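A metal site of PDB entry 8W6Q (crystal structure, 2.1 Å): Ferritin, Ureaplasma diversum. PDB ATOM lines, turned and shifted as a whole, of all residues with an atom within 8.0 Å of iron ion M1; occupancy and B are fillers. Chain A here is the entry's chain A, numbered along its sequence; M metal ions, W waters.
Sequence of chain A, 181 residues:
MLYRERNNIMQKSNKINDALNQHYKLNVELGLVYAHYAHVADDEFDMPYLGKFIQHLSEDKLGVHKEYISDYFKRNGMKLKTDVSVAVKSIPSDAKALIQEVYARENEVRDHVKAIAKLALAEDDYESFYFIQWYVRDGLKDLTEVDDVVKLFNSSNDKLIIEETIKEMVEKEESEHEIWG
Water W1 bridges OD1 of Asp 60 (3.0 Å) and OD1 of Asp 138 (3.2 Å).
Four residues have an atom within 4 Å of iron ion M1: Asp 60, His 65, Asp 138 and Asp 142.
Iron ion M1 is bound by OD2 of Asp 138 (2.0 Å), NE2 of His 65 (2.2 Å), OD2 of Asp 60 (2.2 Å), water W2 (2.3 Å), water W1 (2.4 Å) and OD2 of Asp 142 (2.4 Å).
Iron ion M1 has six donor atoms within binding distance.
Slightly farther from iron ion M1 lies the side-chain carboxylate (OD1) of Asp 142 (2.8 Å).
The guanidinium group (NH2) of Arg 137 lies within salt-bridge range of the side-chain carboxylate (OD1) of Asp 138 (3.0 Å).
OD1 of Asn 27 sits close to ND1 of His 65 (3.4 Å).
The backbone carbonyl oxygen (O) of His 65 is in hydrogen-bond range of the side-chain hydroxyl (OH) of Tyr 135, at 2.6 Å.
The side-chain carboxylate (OD2) of Asp 142 sits close to the side-chain amino group (NZ) of Lys 61, at 3.4 Å.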
ATOM      1  N   ASN A  27     -17.744 -38.230  -2.867  1.00  0.00           N
ATOM      2  CA  ASN A  27     -16.738 -37.190  -3.093  1.00  0.00           C
ATOM      3  C   ASN A  27     -15.742 -37.597  -4.168  1.00  0.00           C
ATOM      4  O   ASN A  27     -15.275 -36.739  -4.936  1.00  0.00           O
ATOM      5  CB  ASN A  27     -16.031 -36.860  -1.798  1.00  0.00           C
ATOM      6  CG  ASN A  27     -16.762 -35.815  -1.019  1.00  0.00           C
ATOM      7  OD1 ASN A  27     -16.725 -34.644  -1.361  1.00  0.00           O
ATOM      8  ND2 ASN A  27     -17.472 -36.231   0.023  1.00  0.00           N
ATOM      9  N   HIS A  56     -10.810 -26.556  -9.485  1.00  0.00           N
ATOM     10  CA  HIS A  56     -10.473 -26.389  -8.074  1.00  0.00           C
ATOM     11  C   HIS A  56     -11.464 -27.125  -7.184  1.00  0.00           C
ATOM     12  O   HIS A  56     -11.087 -27.712  -6.171  1.00  0.00           O
ATOM     13  CB  HIS A  56     -10.433 -24.905  -7.700  1.00  0.00           C
ATOM     14  CG  HIS A  56     -10.120 -24.661  -6.260  1.00  0.00           C
ATOM     15  ND1 HIS A  56     -11.094 -24.319  -5.332  1.00  0.00           N
ATOM     16  CD2 HIS A  56      -8.960 -24.705  -5.574  1.00  0.00           C
ATOM     17  CE1 HIS A  56     -10.535 -24.169  -4.145  1.00  0.00           C
ATOM     18  NE2 HIS A  56      -9.236 -24.396  -4.260  1.00  0.00           N
ATOM     19  N   LEU A  57     -12.751 -27.073  -7.537  1.00  0.00           N
ATOM     20  CA  LEU A  57     -13.747 -27.877  -6.825  1.00  0.00           C
ATOM     21  C   LEU A  57     -13.473 -29.367  -6.983  1.00  0.00           C
ATOM     22  O   LEU A  57     -13.646 -30.143  -6.031  1.00  0.00           O
ATOM     23  CB  LEU A  57     -15.140 -27.517  -7.328  1.00  0.00           C
ATOM     24  CG  LEU A  57     -15.880 -26.555  -6.428  1.00  0.00           C
ATOM     25  CD1 LEU A  57     -15.037 -25.319  -6.111  1.00  0.00           C
ATOM     26  CD2 LEU A  57     -17.173 -26.189  -7.122  1.00  0.00           C
ATOM     27  N   GLU A  59     -10.573 -30.760  -7.211  1.00  0.00           N
ATOM     28  CA  GLU A  59      -9.461 -31.119  -6.349  1.00  0.00           C
ATOM     29  C   GLU A  59      -9.827 -31.073  -4.873  1.00  0.00           C
ATOM     30  O   GLU A  59      -9.227 -31.794  -4.060  1.00  0.00           O
ATOM     31  CB  GLU A  59      -8.288 -30.216  -6.678  1.00  0.00           C
ATOM     32  CG  GLU A  59      -7.744 -30.524  -8.074  1.00  0.00           C
ATOM     33  CD  GLU A  59      -6.869 -29.413  -8.622  1.00  0.00           C
ATOM     34  OE1 GLU A  59      -6.468 -29.499  -9.815  1.00  0.00           O
ATOM     35  OE2 GLU A  59      -6.621 -28.453  -7.882  1.00  0.00           O
ATOM     36  N   ASP A  60     -10.820 -30.248  -4.504  1.00  0.00           N
ATOM     37  CA  ASP A  60     -11.315 -30.242  -3.139  1.00  0.00           C
ATOM     38  C   ASP A  60     -12.012 -31.558  -2.809  1.00  0.00           C
ATOM     39  O   ASP A  60     -11.784 -32.137  -1.743  1.00  0.00           O
ATOM     40  CB  ASP A  60     -12.269 -29.069  -2.935  1.00  0.00           C
ATOM     41  CG  ASP A  60     -12.525 -28.779  -1.477  1.00  0.00           C
ATOM     42  OD1 ASP A  60     -11.834 -29.366  -0.612  1.00  0.00           O
ATOM     43  OD2 ASP A  60     -13.407 -27.951  -1.178  1.00  0.00           O
ATOM     44  N   LYS A  61     -12.864 -32.043  -3.717  1.00  0.00           N
ATOM     45  CA  LYS A  61     -13.602 -33.277  -3.458  1.00  0.00           C
ATOM     46  C   LYS A  61     -12.657 -34.477  -3.388  1.00  0.00           C
ATOM     47  O   LYS A  61     -12.753 -35.303  -2.470  1.00  0.00           O
ATOM     48  CB  LYS A  61     -14.650 -33.505  -4.558  1.00  0.00           C
ATOM     49  CG  LYS A  61     -15.646 -32.385  -4.774  1.00  0.00           C
ATOM     50  CD  LYS A  61     -16.332 -31.953  -3.481  1.00  0.00           C
ATOM     51  CE  LYS A  61     -17.426 -30.927  -3.761  1.00  0.00           C
ATOM     52  NZ  LYS A  61     -18.209 -30.590  -2.531  1.00  0.00           N
ATOM     53  N   VAL A  64      -9.152 -32.908   0.325  1.00  0.00           N
ATOM     54  CA  VAL A  64      -9.433 -32.965   1.757  1.00  0.00           C
ATOM     55  C   VAL A  64     -10.777 -33.620   2.051  1.00  0.00           C
ATOM     56  O   VAL A  64     -10.951 -34.249   3.099  1.00  0.00           O
ATOM     57  CB  VAL A  64      -9.330 -31.565   2.394  1.00  0.00           C
ATOM     58  CG1 VAL A  64      -7.885 -31.055   2.313  1.00  0.00           C
ATOM     59  CG2 VAL A  64     -10.292 -30.595   1.744  1.00  0.00           C
ATOM     60  N   HIS A  65     -11.749 -33.489   1.148  1.00  0.00           N
ATOM     61  CA  HIS A  65     -13.069 -34.058   1.418  1.00  0.00           C
ATOM     62  C   HIS A  65     -13.008 -35.567   1.646  1.00  0.00           C
ATOM     63  O   HIS A  65     -13.636 -36.085   2.581  1.00  0.00           O
ATOM     64  CB  HIS A  65     -14.028 -33.751   0.276  1.00  0.00           C
ATOM     65  CG  HIS A  65     -14.687 -32.416   0.399  1.00  0.00           C
ATOM     66  ND1 HIS A  65     -15.961 -32.273   0.900  1.00  0.00           N
ATOM     67  CD2 HIS A  65     -14.261 -31.173   0.076  1.00  0.00           C
ATOM     68  CE1 HIS A  65     -16.303 -30.990   0.875  1.00  0.00           C
ATOM     69  NE2 HIS A  65     -15.291 -30.307   0.372  1.00  0.00           N
ATOM     70  N   GLU A 106     -24.078 -29.841  -5.524  1.00  0.00           N
ATOM     71  CA  GLU A 106     -23.642 -29.340  -4.207  1.00  0.00           C
ATOM     72  C   GLU A 106     -24.808 -29.243  -3.233  1.00  0.00           C
ATOM     73  O   GLU A 106     -24.636 -29.453  -2.029  1.00  0.00           O
ATOM     74  CB  GLU A 106     -22.960 -27.973  -4.345  1.00  0.00           C
ATOM     75  CG  GLU A 106     -21.628 -27.984  -5.092  1.00  0.00           C
ATOM     76  CD  GLU A 106     -20.595 -28.888  -4.442  1.00  0.00           C
ATOM     77  OE1 GLU A 106     -20.452 -28.837  -3.199  1.00  0.00           O
ATOM     78  OE2 GLU A 106     -19.933 -29.629  -5.180  1.00  0.00           O
ATOM     79  N   VAL A 109     -25.214 -32.473  -1.728  1.00  0.00           N
ATOM     80  CA  VAL A 109     -24.217 -32.718  -0.696  1.00  0.00           C
ATOM     81  C   VAL A 109     -24.734 -32.257   0.651  1.00  0.00           C
ATOM     82  O   VAL A 109     -24.668 -33.000   1.645  1.00  0.00           O
ATOM     83  CB  VAL A 109     -22.861 -32.064  -1.057  1.00  0.00           C
ATOM     84  CG1 VAL A 109     -21.929 -32.082   0.171  1.00  0.00           C
ATOM     85  CG2 VAL A 109     -22.191 -32.802  -2.239  1.00  0.00           C
ATOM     86  N   TRP A 134     -17.389 -30.148  10.146  1.00  0.00           N
ATOM     87  CA  TRP A 134     -16.608 -29.616   9.031  1.00  0.00           C
ATOM     88  C   TRP A 134     -17.388 -29.698   7.734  1.00  0.00           C
ATOM     89  O   TRP A 134     -17.431 -28.741   6.952  1.00  0.00           O
ATOM     90  CB  TRP A 134     -15.276 -30.373   8.906  1.00  0.00           C
ATOM     91  CG  TRP A 134     -14.313 -29.772   7.910  1.00  0.00           C
ATOM     92  CD1 TRP A 134     -13.313 -28.870   8.168  1.00  0.00           C
ATOM     93  CD2 TRP A 134     -14.250 -30.044   6.496  1.00  0.00           C
ATOM     94  NE1 TRP A 134     -12.637 -28.551   7.007  1.00  0.00           N
ATOM     95  CE2 TRP A 134     -13.185 -29.267   5.964  1.00  0.00           C
ATOM     96  CE3 TRP A 134     -14.988 -30.864   5.624  1.00  0.00           C
ATOM     97  CZ2 TRP A 134     -12.846 -29.262   4.609  1.00  0.00           C
ATOM     98  CZ3 TRP A 134     -14.644 -30.871   4.263  1.00  0.00           C
ATOM     99  CH2 TRP A 134     -13.585 -30.087   3.774  1.00  0.00           C
ATOM    100  N   TYR A 135     -18.037 -30.840   7.501  1.00  0.00           N
ATOM    101  CA  TYR A 135     -18.800 -31.034   6.276  1.00  0.00           C
ATOM    102  C   TYR A 135     -20.111 -30.264   6.301  1.00  0.00           C
ATOM    103  O   TYR A 135     -20.605 -29.870   5.242  1.00  0.00           O
ATOM    104  CB  TYR A 135     -19.039 -32.533   6.061  1.00  0.00           C
ATOM    105  CG  TYR A 135     -17.743 -33.289   5.797  1.00  0.00           C
ATOM    106  CD1 TYR A 135     -16.897 -33.665   6.844  1.00  0.00           C
ATOM    107  CD2 TYR A 135     -17.363 -33.611   4.511  1.00  0.00           C
ATOM    108  CE1 TYR A 135     -15.707 -34.350   6.603  1.00  0.00           C
ATOM    109  CE2 TYR A 135     -16.175 -34.298   4.255  1.00  0.00           C
ATOM    110  CZ  TYR A 135     -15.357 -34.672   5.307  1.00  0.00           C
ATOM    111  OH  TYR A 135     -14.169 -35.349   5.050  1.00  0.00           O
ATOM    112  N   ARG A 137     -20.405 -27.215   7.687  1.00  0.00           N
ATOM    113  CA  ARG A 137     -19.970 -25.878   7.327  1.00  0.00           C
ATOM    114  C   ARG A 137     -19.565 -25.814   5.858  1.00  0.00           C
ATOM    115  O   ARG A 137     -19.954 -24.889   5.132  1.00  0.00           O
ATOM    116  CB  ARG A 137     -18.814 -25.443   8.227  1.00  0.00           C
ATOM    117  CG  ARG A 137     -18.202 -24.089   7.841  1.00  0.00           C
ATOM    118  CD  ARG A 137     -16.714 -23.983   8.246  1.00  0.00           C
ATOM    119  NE  ARG A 137     -15.947 -25.151   7.806  1.00  0.00           N
ATOM    120  CZ  ARG A 137     -15.568 -25.367   6.548  1.00  0.00           C
ATOM    121  NH1 ARG A 137     -15.867 -24.482   5.595  1.00  0.00           N
ATOM    122  NH2 ARG A 137     -14.891 -26.460   6.228  1.00  0.00           N
ATOM    123  N   ASP A 138     -18.782 -26.790   5.416  1.00  0.00           N
ATOM    124  CA  ASP A 138     -18.282 -26.745   4.056  1.00  0.00           C
ATOM    125  C   ASP A 138     -19.403 -26.976   3.042  1.00  0.00           C
ATOM    126  O   ASP A 138     -19.311 -26.486   1.912  1.00  0.00           O
ATOM    127  CB  ASP A 138     -17.187 -27.786   3.904  1.00  0.00           C
ATOM    128  CG  ASP A 138     -16.138 -27.363   2.904  1.00  0.00           C
ATOM    129  OD1 ASP A 138     -15.340 -26.475   3.256  1.00  0.00           O
ATOM    130  OD2 ASP A 138     -16.095 -27.931   1.798  1.00  0.00           O
ATOM    131  N   GLY A 139     -20.465 -27.685   3.426  1.00  0.00           N
ATOM    132  CA  GLY A 139     -21.598 -27.857   2.528  1.00  0.00           C
ATOM    133  C   GLY A 139     -22.186 -26.520   2.102  1.00  0.00           C
ATOM    134  O   GLY A 139     -22.410 -26.283   0.918  1.00  0.00           O
ATOM    135  N   LYS A 141     -20.660 -23.454   2.590  1.00  0.00           N
ATOM    136  CA  LYS A 141     -19.617 -22.637   1.983  1.00  0.00           C
ATOM    137  C   LYS A 141     -19.463 -22.966   0.497  1.00  0.00           C
ATOM    138  O   LYS A 141     -19.398 -22.065  -0.346  1.00  0.00           O
ATOM    139  CB  LYS A 141     -18.284 -22.819   2.695  1.00  0.00           C
ATOM    140  CG  LYS A 141     -17.135 -22.024   2.045  1.00  0.00           C
ATOM    141  CD  LYS A 141     -15.766 -22.643   2.307  1.00  0.00           C
ATOM    142  CE  LYS A 141     -14.648 -21.675   1.912  1.00  0.00           C
ATOM    143  NZ  LYS A 141     -13.279 -22.196   2.218  1.00  0.00           N
ATOM    144  N   ASP A 142     -19.394 -24.267   0.166  1.00  0.00           N
ATOM    145  CA  ASP A 142     -19.246 -24.692  -1.218  1.00  0.00           C
ATOM    146  C   ASP A 142     -20.440 -24.243  -2.058  1.00  0.00           C
ATOM    147  O   ASP A 142     -20.257 -23.780  -3.191  1.00  0.00           O
ATOM    148  CB  ASP A 142     -19.092 -26.205  -1.309  1.00  0.00           C
ATOM    149  CG  ASP A 142     -17.723 -26.697  -0.885  1.00  0.00           C
ATOM    150  OD1 ASP A 142     -16.769 -25.889  -0.866  1.00  0.00           O
ATOM    151  OD2 ASP A 142     -17.602 -27.903  -0.573  1.00  0.00           O
ATOM    152  N   LEU A 143     -21.660 -24.426  -1.541  1.00  0.00           N
ATOM    153  CA  LEU A 143     -22.830 -23.973  -2.277  1.00  0.00           C
ATOM    154  C   LEU A 143     -22.776 -22.477  -2.544  1.00  0.00           C
ATOM    155  O   LEU A 143     -23.134 -22.027  -3.642  1.00  0.00           O
ATOM    156  CB  LEU A 143     -24.113 -24.338  -1.521  1.00  0.00           C
ATOM    157  CG  LEU A 143     -25.366 -24.044  -2.335  1.00  0.00           C
ATOM    158  CD1 LEU A 143     -25.652 -25.222  -3.247  1.00  0.00           C
ATOM    159  CD2 LEU A 143     -26.560 -23.775  -1.439  1.00  0.00           C
ATOM    160  N   GLU A 145     -20.167 -20.544  -2.875  1.00  0.00           N
ATOM    161  CA  GLU A 145     -19.188 -20.257  -3.923  1.00  0.00           C
ATOM    162  C   GLU A 145     -19.741 -20.587  -5.296  1.00  0.00           C
ATOM    163  O   GLU A 145     -19.519 -19.824  -6.247  1.00  0.00           O
ATOM    164  CB  GLU A 145     -17.901 -21.037  -3.689  1.00  0.00           C
ATOM    165  CG  GLU A 145     -17.076 -20.526  -2.556  1.00  0.00           C
ATOM    166  CD  GLU A 145     -15.723 -21.225  -2.490  1.00  0.00           C
ATOM    167  OE1 GLU A 145     -15.485 -22.156  -3.309  1.00  0.00           O
ATOM    168  OE2 GLU A 145     -14.913 -20.825  -1.620  1.00  0.00           O
HETATM  169 FE    FE M   1     -15.290 -28.150  -0.039  1.00  0.00          FE
HETATM  170 FE    FE M   2     -11.733 -23.202  -1.877  1.00  0.00          FE
HETATM  171  O   HOH W   1     -13.327 -27.278   0.921  1.00  0.00           O
HETATM  172  O   HOH W   2     -15.413 -28.274  -2.340  1.00  0.00           O
